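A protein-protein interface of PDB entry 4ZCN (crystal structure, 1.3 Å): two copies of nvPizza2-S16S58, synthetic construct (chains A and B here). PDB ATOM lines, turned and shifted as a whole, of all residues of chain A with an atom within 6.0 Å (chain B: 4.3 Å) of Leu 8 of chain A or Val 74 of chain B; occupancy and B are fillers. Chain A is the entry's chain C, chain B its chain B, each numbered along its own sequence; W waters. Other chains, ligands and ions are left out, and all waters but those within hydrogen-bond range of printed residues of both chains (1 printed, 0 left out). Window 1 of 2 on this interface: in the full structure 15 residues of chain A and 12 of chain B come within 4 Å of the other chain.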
ATOM      1  N   PHE A   5      -9.106  35.241 -19.023  1.00  0.00           N
ATOM      2  CA  PHE A   5      -8.731  34.572 -17.770  1.00  0.00           C
ATOM      3  C   PHE A   5      -7.558  35.365 -17.215  1.00  0.00           C
ATOM      4  O   PHE A   5      -6.729  35.872 -17.975  1.00  0.00           O
ATOM      5  CB  PHE A   5      -8.336  33.096 -17.948  1.00  0.00           C
ATOM      6  CG  PHE A   5      -9.503  32.133 -17.980  1.00  0.00           C
ATOM      7  CD1 PHE A   5     -10.378  32.028 -16.906  1.00  0.00           C
ATOM      8  CD2 PHE A   5      -9.702  31.307 -19.075  1.00  0.00           C
ATOM      9  CE1 PHE A   5     -11.443  31.130 -16.938  1.00  0.00           C
ATOM     10  CE2 PHE A   5     -10.761  30.404 -19.112  1.00  0.00           C
ATOM     11  CZ  PHE A   5     -11.630  30.313 -18.049  1.00  0.00           C
ATOM     12  N   THR A   6      -7.494  35.482 -15.896  1.00  0.00           N
ATOM     13  CA  THR A   6      -6.508  36.334 -15.251  1.00  0.00           C
ATOM     14  C   THR A   6      -5.889  35.628 -14.051  1.00  0.00           C
ATOM     15  O   THR A   6      -6.598  35.008 -13.263  1.00  0.00           O
ATOM     16  CB  THR A   6      -7.156  37.679 -14.802  1.00  0.00           C
ATOM     17  OG1 THR A   6      -7.294  38.540 -15.938  1.00  0.00           O
ATOM     18  CG2 THR A   6      -6.312  38.398 -13.732  1.00  0.00           C
ATOM     19  N   GLY A   7      -4.570  35.714 -13.914  1.00  0.00           N
ATOM     20  CA  GLY A   7      -3.921  35.290 -12.690  1.00  0.00           C
ATOM     21  C   GLY A   7      -3.876  33.787 -12.503  1.00  0.00           C
ATOM     22  O   GLY A   7      -3.781  33.312 -11.382  1.00  0.00           O
ATOM     23  N   LEU A   8      -3.925  33.022 -13.588  1.00  0.00           N
ATOM     24  CA  LEU A   8      -3.811  31.572 -13.448  1.00  0.00           C
ATOM     25  C   LEU A   8      -2.382  31.155 -13.150  1.00  0.00           C
ATOM     26  O   LEU A   8      -1.424  31.775 -13.613  1.00  0.00           O
ATOM     27  CB  LEU A   8      -4.281  30.846 -14.708  1.00  0.00           C
ATOM     28  CG  LEU A   8      -5.684  31.122 -15.239  1.00  0.00           C
ATOM     29  CD1 LEU A   8      -5.919  30.292 -16.501  1.00  0.00           C
ATOM     30  CD2 LEU A   8      -6.757  30.848 -14.205  1.00  0.00           C
ATOM     31  N   ASN A   9      -2.245  30.079 -12.393  1.00  0.00           N
ATOM     32  CA  ASN A   9      -0.949  29.457 -12.199  1.00  0.00           C
ATOM     33  C   ASN A   9      -1.079  27.957 -12.308  1.00  0.00           C
ATOM     34  O   ASN A   9      -1.916  27.353 -11.634  1.00  0.00           O
ATOM     35  CB  ASN A   9      -0.351  29.841 -10.847  1.00  0.00           C
ATOM     36  CG  ASN A   9       0.097  31.284 -10.809  1.00  0.00           C
ATOM     37  OD1 ASN A   9      -0.642  32.156 -10.356  1.00  0.00           O
ATOM     38  ND2 ASN A   9       1.301  31.550 -11.308  1.00  0.00           N
ATOM     39  N   THR A  10      -0.243  27.379 -13.171  1.00  0.00           N
ATOM     40  CA  THR A  10      -0.226  25.950 -13.484  1.00  0.00           C
ATOM     41  C   THR A  10      -1.628  25.336 -13.521  1.00  0.00           C
ATOM     42  O   THR A  10      -1.900  24.360 -12.815  1.00  0.00           O
ATOM     43  CB  THR A  10       0.673  25.162 -12.485  1.00  0.00           C
ATOM     44  OG1 THR A  10       0.266  25.422 -11.139  1.00  0.00           O
ATOM     45  CG2 THR A  10       2.142  25.553 -12.657  1.00  0.00           C
ATOM     46  N   PRO A  11      -2.526  25.893 -14.357  1.00  0.00           N
ATOM     47  CA  PRO A  11      -3.880  25.333 -14.460  1.00  0.00           C
ATOM     48  C   PRO A  11      -3.839  23.863 -14.869  1.00  0.00           C
ATOM     49  O   PRO A  11      -3.039  23.491 -15.733  1.00  0.00           O
ATOM     50  CB  PRO A  11      -4.543  26.196 -15.542  1.00  0.00           C
ATOM     51  CG  PRO A  11      -3.385  26.717 -16.365  1.00  0.00           C
ATOM     52  CD  PRO A  11      -2.287  26.942 -15.368  1.00  0.00           C
ATOM     53  N   VAL A  14      -9.657  21.544 -17.646  1.00  0.00           N
ATOM     54  CA  VAL A  14     -10.673  22.404 -18.235  1.00  0.00           C
ATOM     55  C   VAL A  14     -11.918  21.587 -18.609  1.00  0.00           C
ATOM     56  O   VAL A  14     -11.808  20.430 -19.001  1.00  0.00           O
ATOM     57  CB  VAL A  14     -10.108  23.140 -19.489  1.00  0.00           C
ATOM     58  CG1 VAL A  14      -9.527  22.143 -20.521  1.00  0.00           C
ATOM     59  CG2 VAL A  14     -11.149  24.054 -20.117  1.00  0.00           C
ATOM     60  N   VAL A  22     -16.697  27.991 -19.798  1.00  0.00           N
ATOM     61  CA  VAL A  22     -15.450  27.264 -19.624  1.00  0.00           C
ATOM     62  C   VAL A  22     -15.034  27.291 -18.159  1.00  0.00           C
ATOM     63  O   VAL A  22     -15.006  28.355 -17.551  1.00  0.00           O
ATOM     64  CB  VAL A  22     -14.334  27.871 -20.502  1.00  0.00           C
ATOM     65  CG1 VAL A  22     -13.028  27.130 -20.292  1.00  0.00           C
ATOM     66  CG2 VAL A  22     -14.740  27.851 -21.991  1.00  0.00           C
ATOM     67  N   VAL A  24     -12.099  26.094 -15.283  1.00  0.00           N
ATOM     68  CA  VAL A  24     -10.689  25.757 -15.174  1.00  0.00           C
ATOM     69  C   VAL A  24     -10.289  25.556 -13.728  1.00  0.00           C
ATOM     70  O   VAL A  24     -10.603  26.391 -12.861  1.00  0.00           O
ATOM     71  CB  VAL A  24      -9.807  26.854 -15.785  1.00  0.00           C
ATOM     72  CG1 VAL A  24      -8.333  26.532 -15.587  1.00  0.00           C
ATOM     73  CG2 VAL A  24     -10.145  27.046 -17.253  1.00  0.00           C
ATOM     74  N   ASP A  26      -7.691  26.128 -11.347  1.00  0.00           N
ATOM     75  CA  ASP A  26      -6.515  26.975 -11.218  1.00  0.00           C
ATOM     76  C   ASP A  26      -5.660  26.420 -10.088  1.00  0.00           C
ATOM     77  O   ASP A  26      -5.646  26.922  -8.958  1.00  0.00           O
ATOM     78  CB  ASP A  26      -6.903  28.427 -10.962  1.00  0.00           C
ATOM     79  CG  ASP A  26      -5.717  29.369 -11.047  1.00  0.00           C
ATOM     80  OD1 ASP A  26      -4.662  28.956 -11.562  1.00  0.00           O
ATOM     81  OD2 ASP A  26      -5.826  30.522 -10.579  1.00  0.00           O
ATOM     82  N   ASN A  29      -3.404  28.204  -7.548  1.00  0.00           N
ATOM     83  CA  ASN A  29      -4.075  29.151  -6.657  1.00  0.00           C
ATOM     84  C   ASN A  29      -5.269  28.579  -5.894  1.00  0.00           C
ATOM     85  O   ASN A  29      -6.071  29.329  -5.330  1.00  0.00           O
ATOM     86  CB  ASN A  29      -4.507  30.374  -7.460  1.00  0.00           C
ATOM     87  CG  ASN A  29      -3.331  31.117  -8.022  1.00  0.00           C
ATOM     88  OD1 ASN A  29      -2.388  31.420  -7.297  1.00  0.00           O
ATOM     89  ND2 ASN A  29      -3.351  31.375  -9.323  1.00  0.00           N
ATOM     90  N   ARG A  31      -8.152  27.240  -6.549  1.00  0.00           N
ATOM     91  CA  ARG A  31      -9.477  27.740  -6.867  1.00  0.00           C
ATOM     92  C   ARG A  31      -9.931  27.216  -8.219  1.00  0.00           C
ATOM     93  O   ARG A  31      -9.117  26.685  -8.997  1.00  0.00           O
ATOM     94  CB  ARG A  31      -9.493  29.271  -6.863  1.00  0.00           C
ATOM     95  CG  ARG A  31      -8.670  29.856  -7.991  1.00  0.00           C
ATOM     96  CD  ARG A  31      -8.569  31.381  -7.945  1.00  0.00           C
ATOM     97  NE  ARG A  31      -7.763  31.840  -9.077  1.00  0.00           N
ATOM     98  CZ  ARG A  31      -7.709  33.091  -9.518  1.00  0.00           C
ATOM     99  NH1 ARG A  31      -8.396  34.060  -8.921  1.00  0.00           N
ATOM    100  NH2 ARG A  31      -6.952  33.377 -10.568  1.00  0.00           N
ATOM    101  N   VAL A  33     -12.133  28.606 -11.572  1.00  0.00           N
ATOM    102  CA  VAL A  33     -12.674  29.812 -12.187  1.00  0.00           C
ATOM    103  C   VAL A  33     -13.468  29.440 -13.421  1.00  0.00           C
ATOM    104  O   VAL A  33     -13.203  28.424 -14.061  1.00  0.00           O
ATOM    105  CB  VAL A  33     -11.563  30.813 -12.550  1.00  0.00           C
ATOM    106  CG1 VAL A  33     -10.838  31.270 -11.290  1.00  0.00           C
ATOM    107  CG2 VAL A  33     -10.579  30.215 -13.534  1.00  0.00           C
ATOM    108  N   GLN A  42     -13.726  36.859 -15.353  1.00  0.00           N
ATOM    109  CA  GLN A  42     -13.833  35.508 -14.823  1.00  0.00           C
ATOM    110  C   GLN A  42     -14.517  35.531 -13.467  1.00  0.00           C
ATOM    111  O   GLN A  42     -14.479  36.538 -12.746  1.00  0.00           O
ATOM    112  CB  GLN A  42     -12.458  34.853 -14.705  1.00  0.00           C
ATOM    113  CG  GLN A  42     -11.613  35.422 -13.592  1.00  0.00           C
ATOM    114  CD  GLN A  42     -10.162  34.992 -13.665  1.00  0.00           C
ATOM    115  OE1 GLN A  42      -9.760  34.256 -14.566  1.00  0.00           O
ATOM    116  NE2 GLN A  42      -9.363  35.460 -12.712  1.00  0.00           N
ATOM    117  N   VAL B  66      -7.681  23.677 -24.233  1.00  0.00           N
ATOM    118  CA  VAL B  66      -6.524  23.088 -23.587  1.00  0.00           C
ATOM    119  C   VAL B  66      -6.010  23.993 -22.472  1.00  0.00           C
ATOM    120  O   VAL B  66      -5.895  25.207 -22.663  1.00  0.00           O
ATOM    121  CB  VAL B  66      -5.407  22.817 -24.625  1.00  0.00           C
ATOM    122  CG1 VAL B  66      -4.114  22.410 -23.951  1.00  0.00           C
ATOM    123  CG2 VAL B  66      -5.861  21.742 -25.605  1.00  0.00           C
ATOM    124  N   THR B  67      -5.730  23.411 -21.306  1.00  0.00           N
ATOM    125  CA  THR B  67      -5.011  24.137 -20.276  1.00  0.00           C
ATOM    126  C   THR B  67      -3.523  24.050 -20.590  1.00  0.00           C
ATOM    127  O   THR B  67      -2.894  22.991 -20.502  1.00  0.00           O
ATOM    128  CB  THR B  67      -5.318  23.615 -18.864  1.00  0.00           C
ATOM    129  OG1 THR B  67      -5.436  22.189 -18.875  1.00  0.00           O
ATOM    130  CG2 THR B  67      -6.627  24.206 -18.363  1.00  0.00           C
ATOM    131  N   ASN B  72       0.450  29.114 -18.067  1.00  0.00           N
ATOM    132  CA  ASN B  72      -0.544  29.713 -17.174  1.00  0.00           C
ATOM    133  C   ASN B  72      -1.741  30.292 -17.923  1.00  0.00           C
ATOM    134  O   ASN B  72      -2.199  31.402 -17.637  1.00  0.00           O
ATOM    135  CB  ASN B  72       0.117  30.798 -16.315  1.00  0.00           C
ATOM    136  CG  ASN B  72       1.219  30.244 -15.429  1.00  0.00           C
ATOM    137  OD1 ASN B  72       1.099  29.137 -14.890  1.00  0.00           O
ATOM    138  ND2 ASN B  72       2.300  30.997 -15.286  1.00  0.00           N
ATOM    139  N   ARG B  73      -2.253  29.530 -18.883  1.00  0.00           N
ATOM    140  CA  ARG B  73      -3.312  30.030 -19.744  1.00  0.00           C
ATOM    141  C   ARG B  73      -4.150  28.891 -20.283  1.00  0.00           C
ATOM    142  O   ARG B  73      -3.770  27.720 -20.192  1.00  0.00           O
ATOM    143  CB  ARG B  73      -2.732  30.830 -20.916  1.00  0.00           C
ATOM    144  CG  ARG B  73      -1.953  29.957 -21.894  1.00  0.00           C
ATOM    145  CD  ARG B  73      -1.341  30.767 -23.021  1.00  0.00           C
ATOM    146  NE  ARG B  73      -0.713  29.886 -24.001  1.00  0.00           N
ATOM    147  CZ  ARG B  73      -0.310  30.265 -25.212  1.00  0.00           C
ATOM    148  NH1 ARG B  73      -0.480  31.523 -25.606  1.00  0.00           N
ATOM    149  NH2 ARG B  73       0.244  29.380 -26.035  1.00  0.00           N
ATOM    150  N   VAL B  74      -5.287  29.253 -20.860  1.00  0.00           N
ATOM    151  CA  VAL B  74      -6.165  28.318 -21.539  1.00  0.00           C
ATOM    152  C   VAL B  74      -6.258  28.753 -22.993  1.00  0.00           C
ATOM    153  O   VAL B  74      -6.367  29.947 -23.263  1.00  0.00           O
ATOM    154  CB  VAL B  74      -7.570  28.281 -20.895  1.00  0.00           C
ATOM    155  CG1 VAL B  74      -8.456  27.242 -21.576  1.00  0.00           C
ATOM    156  CG2 VAL B  74      -7.457  28.019 -19.395  1.00  0.00           C
ATOM    157  N   VAL B  75      -6.186  27.809 -23.926  1.00  0.00           N
ATOM    158  CA  VAL B  75      -6.320  28.138 -25.339  1.00  0.00           C
ATOM    159  C   VAL B  75      -7.380  27.263 -25.980  1.00  0.00           C
ATOM    160  O   VAL B  75      -7.695  26.185 -25.465  1.00  0.00           O
ATOM    161  CB  VAL B  75      -4.980  27.977 -26.095  1.00  0.00           C
ATOM    162  CG1 VAL B  75      -3.934  28.954 -25.557  1.00  0.00           C
ATOM    163  CG2 VAL B  75      -4.472  26.556 -25.999  1.00  0.00           C
ATOM    164  N   VAL B  86      -6.517  32.548 -27.418  1.00  0.00           N
ATOM    165  CA  VAL B  86      -6.232  32.495 -25.992  1.00  0.00           C
ATOM    166  C   VAL B  86      -7.448  32.976 -25.213  1.00  0.00           C
ATOM    167  O   VAL B  86      -7.976  34.049 -25.495  1.00  0.00           O
ATOM    168  CB  VAL B  86      -5.015  33.356 -25.619  1.00  0.00           C
ATOM    169  CG1 VAL B  86      -4.772  33.308 -24.114  1.00  0.00           C
ATOM    170  CG2 VAL B  86      -3.791  32.892 -26.391  1.00  0.00           C
ATOM    171  N   LEU B  87      -7.899  32.194 -24.232  1.00  0.00           N
ATOM    172  CA  LEU B  87      -9.102  32.554 -23.471  1.00  0.00           C
ATOM    173  C   LEU B  87      -8.828  33.546 -22.351  1.00  0.00           C
ATOM    174  O   LEU B  87      -7.769  33.512 -21.725  1.00  0.00           O
ATOM    175  CB  LEU B  87      -9.762  31.309 -22.879  1.00  0.00           C
ATOM    176  CG  LEU B  87     -10.626  30.441 -23.796  1.00  0.00           C
ATOM    177  CD1 LEU B  87      -9.775  29.667 -24.781  1.00  0.00           C
ATOM    178  CD2 LEU B  87     -11.455  29.498 -22.960  1.00  0.00           C
ATOM    179  OXT LEU B  87      -9.680  34.385 -22.043  1.00  0.00           O
HETATM  180  O   HOH W   1      -3.240  33.717 -16.462  1.00  0.00           O
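The side-chain amide oxygen (OD1) of Asn 72 of chain B is in hydrogen-bond range of the backbone NH (N) of Thr 10 of chain A (2.8 Å).
OXT of Leu 87 of chain B lies within hydrogen-bond range of N of Phe 5 of chain A.
The backbone carbonyl oxygen of Val 74 of chain B is in hydrogen-bond range of the backbone NH of Leu 87 of chain B (2.9 Å).
ND2 of Asn 29 of chain A is in hydrogen-bond range of OD1 of Asn 9 of chain A, 3.0 Å away.
The side-chain amide oxygen of Asn 9 of chain A sits close to the backbone carbonyl oxygen of Gly 7 of chain A (3.5 Å).
The backbone NH (N) of Asn 9 of chain A is in hydrogen-bond range of the side-chain carboxylate (OD1) of Asp 26 of chain A, at 2.8 Å.
N of Val 24 of chain A sits at hydrogen-bond distance from O of Val 33 of chain A, at 2.9 Å.
Among the printed residues, merely in contact across the chains: Leu 8 of chain A with Asn 72 of chain B (3.3 Å), Asn 9 of chain A with Asn 72 of chain B (3.4 Å), Val 24 of chain A with Val 74 of chain B (3.6 Å), Pro 11 of chain A with Asn 72 of chain B (3.7 Å), Val 22 of chain A with Leu 87 of chain B (3.8 Å), Val 14 of chain A with Thr 67 of chain B (3.8 Å), Pro 11 of chain A with Thr 67 of chain B (3.9 Å), Pro 11 of chain A with Arg 73 of chain B (3.9 Å), Leu 8 of chain A with Val 74 of chain B (3.99 Å) and Phe 5 of chain A with Val 74 of chain B (3.99 Å).
Printed residues of chain B within 4 Å of Leu 8 of chain A: Asn 72 (3.3 Å) and Val 74 (3.99 Å).
Of the printed residues of chain A, Val 74 of chain B touches Phe 5 (3.99 Å), Leu 8 (3.99 Å) and Val 24 (3.6 Å).
Of the printed residues of chain B, Thr 10 of chain A touches Asn 72.
Of the printed residues of chain A, Arg 73 of chain B touches Pro 11.
Of the printed residues of chain B, Pro 11 of chain A touches Thr 67 (3.9 Å), Asn 72 (3.7 Å) and Arg 73 (3.9 Å).
Of the printed residues of chain B, Asn 9 of chain A touches Asn 72.
The nearest printed residue of chain A that does not touch Thr 67 of chain B is Val 24 of chain A (4.003 Å).
Hydrophobic or aromatic side chains of chain A within 4 Å of the printed part of chain B: Phe 5, Leu 8, Pro 11, Val 14, Val 22 and Val 24.
Of the 8 printed residues of chain B, 5 touch a printed residue of chain A.
Printed residues of chain B that touch a printed residue of chain A: Thr 67, Asn 72, Arg 73, Val 74 and Leu 87.
Among the printed residues, no Asp or Glu carboxylate lies within 4 Å of a Lys or Arg side-chain nitrogen of the other chain.
No position is printed for both chains.
Of the 12 pairs that touch across the chains among the printed residues, none has its exchanged pair printed and touching as well.
Water W1 bridges O of Asn 72 of chain B (2.8 Å) and N of Leu 8 of chain A (3.0 Å).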
